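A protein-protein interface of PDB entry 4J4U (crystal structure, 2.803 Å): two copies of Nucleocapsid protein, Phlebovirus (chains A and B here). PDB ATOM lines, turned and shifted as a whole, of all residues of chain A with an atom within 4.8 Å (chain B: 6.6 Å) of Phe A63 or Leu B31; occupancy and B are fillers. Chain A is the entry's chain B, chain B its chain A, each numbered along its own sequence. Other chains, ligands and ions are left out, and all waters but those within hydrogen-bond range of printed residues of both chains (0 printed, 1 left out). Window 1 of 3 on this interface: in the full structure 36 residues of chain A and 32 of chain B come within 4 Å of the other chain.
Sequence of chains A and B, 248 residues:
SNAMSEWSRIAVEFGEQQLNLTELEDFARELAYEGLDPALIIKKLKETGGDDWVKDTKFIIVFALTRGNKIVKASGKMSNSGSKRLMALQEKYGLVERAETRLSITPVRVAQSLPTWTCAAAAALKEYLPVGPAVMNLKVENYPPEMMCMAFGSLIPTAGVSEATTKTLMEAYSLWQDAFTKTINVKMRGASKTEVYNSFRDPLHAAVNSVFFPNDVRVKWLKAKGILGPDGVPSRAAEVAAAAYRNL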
ATOM      1  N   PHE A  59      -0.319 -11.102   8.494  1.00  0.00           N
ATOM      2  CA  PHE A  59       0.308 -12.178   7.733  1.00  0.00           C
ATOM      3  C   PHE A  59      -0.342 -13.514   8.105  1.00  0.00           C
ATOM      4  O   PHE A  59      -0.487 -14.422   7.280  1.00  0.00           O
ATOM      5  CB  PHE A  59       1.821 -12.192   7.985  1.00  0.00           C
ATOM      6  CG  PHE A  59       2.581 -13.120   7.084  1.00  0.00           C
ATOM      7  CD1 PHE A  59       2.719 -14.464   7.398  1.00  0.00           C
ATOM      8  CD2 PHE A  59       3.150 -12.659   5.920  1.00  0.00           C
ATOM      9  CE1 PHE A  59       3.410 -15.335   6.558  1.00  0.00           C
ATOM     10  CE2 PHE A  59       3.838 -13.520   5.077  1.00  0.00           C
ATOM     11  CZ  PHE A  59       3.969 -14.862   5.398  1.00  0.00           C
ATOM     12  N   ILE A  60      -0.744 -13.628   9.362  1.00  0.00           N
ATOM     13  CA  ILE A  60      -1.439 -14.822   9.801  1.00  0.00           C
ATOM     14  C   ILE A  60      -2.840 -14.825   9.190  1.00  0.00           C
ATOM     15  O   ILE A  60      -3.324 -15.858   8.704  1.00  0.00           O
ATOM     16  CB  ILE A  60      -1.475 -14.924  11.342  1.00  0.00           C
ATOM     17  CG1 ILE A  60      -0.063 -15.211  11.870  1.00  0.00           C
ATOM     18  CG2 ILE A  60      -2.481 -15.999  11.815  1.00  0.00           C
ATOM     19  CD1 ILE A  60       0.105 -15.000  13.383  1.00  0.00           C
ATOM     20  N   ILE A  61      -3.476 -13.661   9.189  1.00  0.00           N
ATOM     21  CA  ILE A  61      -4.822 -13.560   8.663  1.00  0.00           C
ATOM     22  C   ILE A  61      -4.881 -13.921   7.172  1.00  0.00           C
ATOM     23  O   ILE A  61      -5.802 -14.607   6.719  1.00  0.00           O
ATOM     24  CB  ILE A  61      -5.478 -12.200   8.962  1.00  0.00           C
ATOM     25  CG1 ILE A  61      -5.612 -11.997  10.472  1.00  0.00           C
ATOM     26  CG2 ILE A  61      -6.860 -12.159   8.371  1.00  0.00           C
ATOM     27  CD1 ILE A  61      -6.548 -10.881  10.894  1.00  0.00           C
ATOM     28  N   VAL A  62      -3.882 -13.495   6.415  1.00  0.00           N
ATOM     29  CA  VAL A  62      -3.863 -13.826   5.002  1.00  0.00           C
ATOM     30  C   VAL A  62      -3.678 -15.336   4.829  1.00  0.00           C
ATOM     31  O   VAL A  62      -4.332 -15.964   3.998  1.00  0.00           O
ATOM     32  CB  VAL A  62      -2.828 -12.979   4.235  1.00  0.00           C
ATOM     33  CG1 VAL A  62      -2.557 -13.538   2.838  1.00  0.00           C
ATOM     34  CG2 VAL A  62      -3.308 -11.542   4.147  1.00  0.00           C
ATOM     35  N   PHE A  63      -2.837 -15.935   5.656  1.00  0.00           N
ATOM     36  CA  PHE A  63      -2.753 -17.389   5.677  1.00  0.00           C
ATOM     37  C   PHE A  63      -4.114 -18.084   5.936  1.00  0.00           C
ATOM     38  O   PHE A  63      -4.460 -19.068   5.280  1.00  0.00           O
ATOM     39  CB  PHE A  63      -1.724 -17.857   6.696  1.00  0.00           C
ATOM     40  CG  PHE A  63      -1.672 -19.343   6.836  1.00  0.00           C
ATOM     41  CD1 PHE A  63      -1.075 -20.120   5.851  1.00  0.00           C
ATOM     42  CD2 PHE A  63      -2.244 -19.972   7.933  1.00  0.00           C
ATOM     43  CE1 PHE A  63      -1.033 -21.505   5.960  1.00  0.00           C
ATOM     44  CE2 PHE A  63      -2.209 -21.358   8.051  1.00  0.00           C
ATOM     45  CZ  PHE A  63      -1.604 -22.125   7.060  1.00  0.00           C
ATOM     46  N   ALA A  64      -4.878 -17.581   6.896  1.00  0.00           N
ATOM     47  CA  ALA A  64      -6.163 -18.190   7.212  1.00  0.00           C
ATOM     48  C   ALA A  64      -7.101 -18.030   6.039  1.00  0.00           C
ATOM     49  O   ALA A  64      -7.829 -18.954   5.683  1.00  0.00           O
ATOM     50  CB  ALA A  64      -6.774 -17.561   8.450  1.00  0.00           C
ATOM     51  N   LEU A  65      -7.068 -16.842   5.443  1.00  0.00           N
ATOM     52  CA  LEU A  65      -7.944 -16.505   4.343  1.00  0.00           C
ATOM     53  C   LEU A  65      -7.748 -17.414   3.141  1.00  0.00           C
ATOM     54  O   LEU A  65      -8.717 -17.869   2.528  1.00  0.00           O
ATOM     55  CB  LEU A  65      -7.736 -15.056   3.950  1.00  0.00           C
ATOM     56  CG  LEU A  65      -8.439 -14.100   4.905  1.00  0.00           C
ATOM     57  CD1 LEU A  65      -8.043 -12.644   4.658  1.00  0.00           C
ATOM     58  CD2 LEU A  65      -9.923 -14.286   4.773  1.00  0.00           C
ATOM     59  N   THR A  66      -6.498 -17.696   2.812  1.00  0.00           N
ATOM     60  CA  THR A  66      -6.216 -18.417   1.588  1.00  0.00           C
ATOM     61  C   THR A  66      -5.811 -19.892   1.761  1.00  0.00           C
ATOM     62  O   THR A  66      -5.779 -20.638   0.786  1.00  0.00           O
ATOM     63  CB  THR A  66      -5.176 -17.657   0.750  1.00  0.00           C
ATOM     64  OG1 THR A  66      -3.931 -17.651   1.445  1.00  0.00           O
ATOM     65  CG2 THR A  66      -5.640 -16.195   0.485  1.00  0.00           C
ATOM     66  N   ARG A  67      -5.525 -20.310   2.996  1.00  0.00           N
ATOM     67  CA  ARG A  67      -5.025 -21.663   3.271  1.00  0.00           C
ATOM     68  C   ARG A  67      -5.722 -22.370   4.423  1.00  0.00           C
ATOM     69  O   ARG A  67      -5.696 -23.593   4.501  1.00  0.00           O
ATOM     70  CB  ARG A  67      -3.528 -21.638   3.546  1.00  0.00           C
ATOM     71  CG  ARG A  67      -2.711 -21.052   2.417  1.00  0.00           C
ATOM     72  CD  ARG A  67      -2.936 -21.833   1.146  1.00  0.00           C
ATOM     73  NE  ARG A  67      -2.434 -23.204   1.220  1.00  0.00           N
ATOM     74  CZ  ARG A  67      -1.359 -23.630   0.563  1.00  0.00           C
ATOM     75  NH1 ARG A  67      -0.673 -22.793  -0.187  1.00  0.00           N
ATOM     76  NH2 ARG A  67      -0.956 -24.888   0.660  1.00  0.00           N
ATOM     77  N   GLY A  68      -6.333 -21.612   5.322  1.00  0.00           N
ATOM     78  CA  GLY A  68      -7.002 -22.211   6.464  1.00  0.00           C
ATOM     79  C   GLY A  68      -6.111 -22.446   7.683  1.00  0.00           C
ATOM     80  O   GLY A  68      -5.289 -21.603   8.031  1.00  0.00           O
ATOM     81  N   ASN A  69      -6.268 -23.605   8.320  1.00  0.00           N
ATOM     82  CA  ASN A  69      -5.686 -23.875   9.628  1.00  0.00           C
ATOM     83  C   ASN A  69      -4.547 -24.890   9.582  1.00  0.00           C
ATOM     84  O   ASN A  69      -3.749 -24.985  10.513  1.00  0.00           O
ATOM     85  CB  ASN A  69      -6.764 -24.372  10.583  1.00  0.00           C
ATOM     86  CG  ASN A  69      -7.529 -23.253  11.260  1.00  0.00           C
ATOM     87  OD1 ASN A  69      -7.000 -22.177  11.516  1.00  0.00           O
ATOM     88  ND2 ASN A  69      -8.789 -23.521  11.580  1.00  0.00           N
ATOM     89  N   LYS A  70      -4.468 -25.656   8.503  1.00  0.00           N
ATOM     90  CA  LYS A  70      -3.519 -26.766   8.449  1.00  0.00           C
ATOM     91  C   LYS A  70      -2.100 -26.334   8.082  1.00  0.00           C
ATOM     92  O   LYS A  70      -1.614 -26.585   6.973  1.00  0.00           O
ATOM     93  CB  LYS A  70      -4.043 -27.920   7.574  1.00  0.00           C
ATOM     94  CG  LYS A  70      -5.025 -28.811   8.326  1.00  0.00           C
ATOM     95  CD  LYS A  70      -5.495 -30.011   7.509  1.00  0.00           C
ATOM     96  CE  LYS A  70      -6.994 -30.253   7.740  1.00  0.00           C
ATOM     97  NZ  LYS A  70      -7.485 -31.593   7.294  1.00  0.00           N
ATOM     98  N   ILE A  71      -1.447 -25.714   9.063  1.00  0.00           N
ATOM     99  CA  ILE A  71      -0.107 -25.111   8.952  1.00  0.00           C
ATOM    100  C   ILE A  71       1.007 -25.995   8.341  1.00  0.00           C
ATOM    101  O   ILE A  71       1.651 -25.612   7.366  1.00  0.00           O
ATOM    102  CB  ILE A  71       0.335 -24.567  10.344  1.00  0.00           C
ATOM    103  CG1 ILE A  71      -0.729 -23.609  10.882  1.00  0.00           C
ATOM    104  CG2 ILE A  71       1.673 -23.859  10.258  1.00  0.00           C
ATOM    105  CD1 ILE A  71      -0.618 -23.287  12.352  1.00  0.00           C
ATOM    106  N   ALA A  74       0.254 -27.203   4.772  1.00  0.00           N
ATOM    107  CA  ALA A  74       0.289 -26.082   3.831  1.00  0.00           C
ATOM    108  C   ALA A  74       1.700 -25.528   3.637  1.00  0.00           C
ATOM    109  O   ALA A  74       2.012 -24.973   2.592  1.00  0.00           O
ATOM    110  CB  ALA A  74      -0.674 -24.978   4.256  1.00  0.00           C
ATOM    111  N   MET A  78       3.945 -24.314  -0.484  1.00  0.00           N
ATOM    112  CA  MET A  78       4.086 -22.892  -0.775  1.00  0.00           C
ATOM    113  C   MET A  78       5.501 -22.501  -1.152  1.00  0.00           C
ATOM    114  O   MET A  78       6.374 -23.336  -1.351  1.00  0.00           O
ATOM    115  CB  MET A  78       3.612 -22.025   0.392  1.00  0.00           C
ATOM    116  CG  MET A  78       4.326 -22.244   1.710  1.00  0.00           C
ATOM    117  SD  MET A  78       3.534 -21.275   3.026  1.00  0.00           S
ATOM    118  CE  MET A  78       1.846 -21.883   2.956  1.00  0.00           C
ATOM    119  N   SER A  79       5.713 -21.201  -1.257  1.00  0.00           N
ATOM    120  CA  SER A  79       7.023 -20.682  -1.578  1.00  0.00           C
ATOM    121  C   SER A  79       7.946 -20.863  -0.375  1.00  0.00           C
ATOM    122  O   SER A  79       7.498 -21.238   0.712  1.00  0.00           O
ATOM    123  CB  SER A  79       6.903 -19.209  -1.935  1.00  0.00           C
ATOM    124  OG  SER A  79       6.528 -18.438  -0.805  1.00  0.00           O
ATOM    125  N   GLY A  82       7.155 -17.887   2.180  1.00  0.00           N
ATOM    126  CA  GLY A  82       5.908 -18.109   2.876  1.00  0.00           C
ATOM    127  C   GLY A  82       6.117 -19.137   3.967  1.00  0.00           C
ATOM    128  O   GLY A  82       5.770 -18.904   5.124  1.00  0.00           O
ATOM    129  N   LEU A  86       5.882 -18.451   7.935  1.00  0.00           N
ATOM    130  CA  LEU A  86       4.748 -19.122   8.602  1.00  0.00           C
ATOM    131  C   LEU A  86       5.160 -20.040   9.749  1.00  0.00           C
ATOM    132  O   LEU A  86       4.596 -19.955  10.844  1.00  0.00           O
ATOM    133  CB  LEU A  86       3.902 -19.918   7.606  1.00  0.00           C
ATOM    134  CG  LEU A  86       2.664 -20.649   8.145  1.00  0.00           C
ATOM    135  CD1 LEU A  86       1.473 -19.724   8.372  1.00  0.00           C
ATOM    136  CD2 LEU A  86       2.296 -21.756   7.201  1.00  0.00           C
ATOM    137  N   PRO A 107      -4.921 -19.956  13.217  1.00  0.00           N
ATOM    138  CA  PRO A 107      -4.935 -18.881  12.225  1.00  0.00           C
ATOM    139  C   PRO A 107      -6.348 -18.355  11.978  1.00  0.00           C
ATOM    140  O   PRO A 107      -6.545 -17.139  12.012  1.00  0.00           O
ATOM    141  CB  PRO A 107      -4.391 -19.566  10.973  1.00  0.00           C
ATOM    142  CG  PRO A 107      -3.449 -20.611  11.496  1.00  0.00           C
ATOM    143  CD  PRO A 107      -4.045 -21.076  12.816  1.00  0.00           C
ATOM    144  N   ASP B  26       1.789  -9.615  -1.944  1.00  0.00           N
ATOM    145  CA  ASP B  26       3.027 -10.374  -1.744  1.00  0.00           C
ATOM    146  C   ASP B  26       2.823 -11.545  -0.800  1.00  0.00           C
ATOM    147  O   ASP B  26       3.273 -12.674  -1.053  1.00  0.00           O
ATOM    148  CB  ASP B  26       4.116  -9.481  -1.142  1.00  0.00           C
ATOM    149  CG  ASP B  26       4.597  -8.415  -2.095  1.00  0.00           C
ATOM    150  OD1 ASP B  26       4.499  -8.627  -3.324  1.00  0.00           O
ATOM    151  OD2 ASP B  26       5.077  -7.366  -1.605  1.00  0.00           O
ATOM    152  N   PHE B  27       2.180 -11.236   0.319  1.00  0.00           N
ATOM    153  CA  PHE B  27       1.833 -12.236   1.303  1.00  0.00           C
ATOM    154  C   PHE B  27       1.011 -13.322   0.609  1.00  0.00           C
ATOM    155  O   PHE B  27       1.260 -14.517   0.787  1.00  0.00           O
ATOM    156  CB  PHE B  27       0.986 -11.628   2.426  1.00  0.00           C
ATOM    157  CG  PHE B  27       1.699 -10.627   3.274  1.00  0.00           C
ATOM    158  CD1 PHE B  27       3.063 -10.376   3.107  1.00  0.00           C
ATOM    159  CD2 PHE B  27       1.000  -9.929   4.257  1.00  0.00           C
ATOM    160  CE1 PHE B  27       3.713  -9.439   3.898  1.00  0.00           C
ATOM    161  CE2 PHE B  27       1.651  -8.985   5.062  1.00  0.00           C
ATOM    162  CZ  PHE B  27       3.010  -8.749   4.878  1.00  0.00           C
ATOM    163  N   ALA B  28       0.029 -12.885  -0.177  1.00  0.00           N
ATOM    164  CA  ALA B  28      -0.880 -13.800  -0.848  1.00  0.00           C
ATOM    165  C   ALA B  28      -0.140 -14.804  -1.719  1.00  0.00           C
ATOM    166  O   ALA B  28      -0.418 -16.014  -1.658  1.00  0.00           O
ATOM    167  CB  ALA B  28      -1.893 -13.028  -1.671  1.00  0.00           C
ATOM    168  N   ARG B  29       0.793 -14.293  -2.525  1.00  0.00           N
ATOM    169  CA  ARG B  29       1.605 -15.133  -3.408  1.00  0.00           C
ATOM    170  C   ARG B  29       2.609 -15.935  -2.596  1.00  0.00           C
ATOM    171  O   ARG B  29       2.818 -17.106  -2.868  1.00  0.00           O
ATOM    172  CB  ARG B  29       2.326 -14.304  -4.477  1.00  0.00           C
ATOM    173  CG  ARG B  29       1.439 -13.325  -5.234  1.00  0.00           C
ATOM    174  CD  ARG B  29       2.129 -12.779  -6.466  1.00  0.00           C
ATOM    175  NE  ARG B  29       2.846 -11.546  -6.174  1.00  0.00           N
ATOM    176  CZ  ARG B  29       2.393 -10.330  -6.475  1.00  0.00           C
ATOM    177  NH1 ARG B  29       1.220 -10.197  -7.083  1.00  0.00           N
ATOM    178  NH2 ARG B  29       3.113  -9.251  -6.179  1.00  0.00           N
ATOM    179  N   GLU B  30       3.221 -15.299  -1.599  1.00  0.00           N
ATOM    180  CA  GLU B  30       4.126 -15.985  -0.684  1.00  0.00           C
ATOM    181  C   GLU B  30       3.459 -17.248  -0.142  1.00  0.00           C
ATOM    182  O   GLU B  30       4.063 -18.321  -0.108  1.00  0.00           O
ATOM    183  CB  GLU B  30       4.527 -15.055   0.472  1.00  0.00           C
ATOM    184  CG  GLU B  30       5.911 -14.402   0.355  1.00  0.00           C
ATOM    185  CD  GLU B  30       6.051 -13.140   1.220  1.00  0.00           C
ATOM    186  OE1 GLU B  30       5.496 -13.129   2.339  1.00  0.00           O
ATOM    187  OE2 GLU B  30       6.697 -12.152   0.777  1.00  0.00           O
ATOM    188  N   LEU B  31       2.189 -17.116   0.236  1.00  0.00           N
ATOM    189  CA  LEU B  31       1.430 -18.194   0.877  1.00  0.00           C
ATOM    190  C   LEU B  31       0.560 -19.030  -0.080  1.00  0.00           C
ATOM    191  O   LEU B  31       0.029 -20.068   0.314  1.00  0.00           O
ATOM    192  CB  LEU B  31       0.570 -17.620   2.006  1.00  0.00           C
ATOM    193  CG  LEU B  31       1.356 -17.119   3.220  1.00  0.00           C
ATOM    194  CD1 LEU B  31       0.563 -16.100   4.010  1.00  0.00           C
ATOM    195  CD2 LEU B  31       1.752 -18.289   4.113  1.00  0.00           C
ATOM    196  N   ALA B  32       0.419 -18.582  -1.327  1.00  0.00           N
ATOM    197  CA  ALA B  32      -0.387 -19.290  -2.325  1.00  0.00           C
ATOM    198  C   ALA B  32       0.087 -20.720  -2.531  1.00  0.00           C
ATOM    199  O   ALA B  32       1.260 -21.027  -2.279  1.00  0.00           O
ATOM    200  CB  ALA B  32      -0.354 -18.567  -3.623  1.00  0.00           C
ATOM    201  N   TYR B  33      -0.819 -21.582  -3.002  1.00  0.00           N
ATOM    202  CA  TYR B  33      -0.501 -22.987  -3.220  1.00  0.00           C
ATOM    203  C   TYR B  33       0.657 -23.111  -4.180  1.00  0.00           C
ATOM    204  O   TYR B  33       0.835 -22.286  -5.068  1.00  0.00           O
ATOM    205  CB  TYR B  33      -1.714 -23.802  -3.719  1.00  0.00           C
ATOM    206  CG  TYR B  33      -1.368 -25.245  -4.048  1.00  0.00           C
ATOM    207  CD1 TYR B  33      -0.865 -25.598  -5.300  1.00  0.00           C
ATOM    208  CD2 TYR B  33      -1.506 -26.243  -3.096  1.00  0.00           C
ATOM    209  CE1 TYR B  33      -0.510 -26.911  -5.583  1.00  0.00           C
ATOM    210  CE2 TYR B  33      -1.169 -27.553  -3.370  1.00  0.00           C
ATOM    211  CZ  TYR B  33      -0.673 -27.881  -4.612  1.00  0.00           C
ATOM    212  OH  TYR B  33      -0.327 -29.182  -4.875  1.00  0.00           O
ATOM    213  N   GLU B  34       1.437 -24.161  -3.987  1.00  0.00           N
ATOM    214  CA  GLU B  34       2.573 -24.446  -4.829  1.00  0.00           C
ATOM    215  C   GLU B  34       2.842 -25.939  -4.748  1.00  0.00           C
ATOM    216  O   GLU B  34       2.972 -26.494  -3.664  1.00  0.00           O
ATOM    217  CB  GLU B  34       3.758 -23.620  -4.344  1.00  0.00           C
ATOM    218  CG  GLU B  34       5.115 -24.161  -4.681  1.00  0.00           C
ATOM    219  CD  GLU B  34       6.177 -23.110  -4.466  1.00  0.00           C
ATOM    220  OE1 GLU B  34       7.312 -23.478  -4.083  1.00  0.00           O
ATOM    221  OE2 GLU B  34       5.858 -21.911  -4.683  1.00  0.00           O
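Of chain B, only Leu B31 (3.8 Å) comes within 4 Å of Phe A63.
Of chain A, only Phe A59, Phe A63, Arg A67 and Met A78 come within 4 Å of Leu B31.
Printed residues of chain A within 4 Å of Glu B30: Phe A59 (3.2 Å), Met A78 (3.8 Å), Ser A79 (2.6 Å) and Gly A82 (3.5 Å).
Of the printed residues of chain A, Ala B32 touches Arg A67 (3.2 Å) and Met A78 (3.7 Å).
Of the printed residues of chain A, Glu B34 touches Met A78 (2.9 Å) and Ser A79 (3.5 Å).
Of the printed residues of chain B, Met A78 touches Glu B30, Leu B31, Ala B32 and Glu B34.
The nearest residue of chain B that does not touch Phe A63 is Phe B27 (6.5 Å).
The nearest printed residue of chain A that does not touch Leu B31 is Gly A82 (4.2 Å).
The nearest printed residue of chain B that does not touch Ser A79 is Arg B29 (4.4 Å).
The side-chain hydroxyl of Ser A79 sits at hydrogen-bond distance from the backbone NH of Gly A82 (3.1 Å).
O of Phe A63 sits at hydrogen-bond distance from N of Gly A68 (3.2 Å).
Phe B27 touches Phe A59 (CD1 to CD2, 3.6 Å).
Phe A59 touches Glu B30 (CE2 to OE1, 3.2 Å).
Leu B31 touches Phe A59.
CD1 of Leu B31 touches N of Phe A63, 3.8 Å away.
Met A78 touches Glu B30 (CB to O, 3.8 Å).
Met A78 touches Leu B31 (SD to CD2, 3.6 Å).
CB of Met A78 touches O of Ala B32, at 3.7 Å.
Ser A79 touches Glu B34.
Glu B30 touches Gly A82 (O to CA, 3.5 Å).
Of the 19 printed residues of chain A, 6 touch a printed residue of chain B.
Printed residues of chain A that touch a printed residue of chain B: Phe A59, Phe A63, Arg A67, Met A78, Ser A79 and Gly A82.
Printed residues of chain B that touch a printed residue of chain A: Phe B27, Glu B30, Leu B31, Ala B32, Tyr B33 and Glu B34.
Among the printed residues, 14 pairs touch across the chains.
Among the printed residues, no Asp or Glu carboxylate lies within 4 Å of a Lys or Arg side-chain nitrogen of the other chain.
The guanidinium group of Arg A67 lies within hydrogen-bond range of the backbone carbonyl oxygen of Leu B31 (2.9 Å).
The side-chain carboxylate (OE1) of Glu B34 sits close to the backbone carbonyl oxygen (O) of Met A78, at 2.9 Å.
NH1 of Arg A67 lies close to O of Ala B32, at 3.4 Å.
The backbone carbonyl oxygen (O) of Glu B30 sits at hydrogen-bond distance from the side-chain hydroxyl (OG) of Ser A79.
The backbone NH (N) of Tyr B33 lies close to the guanidinium group (NH1) of Arg A67, at 3.1 Å.
No position is printed for both chains.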
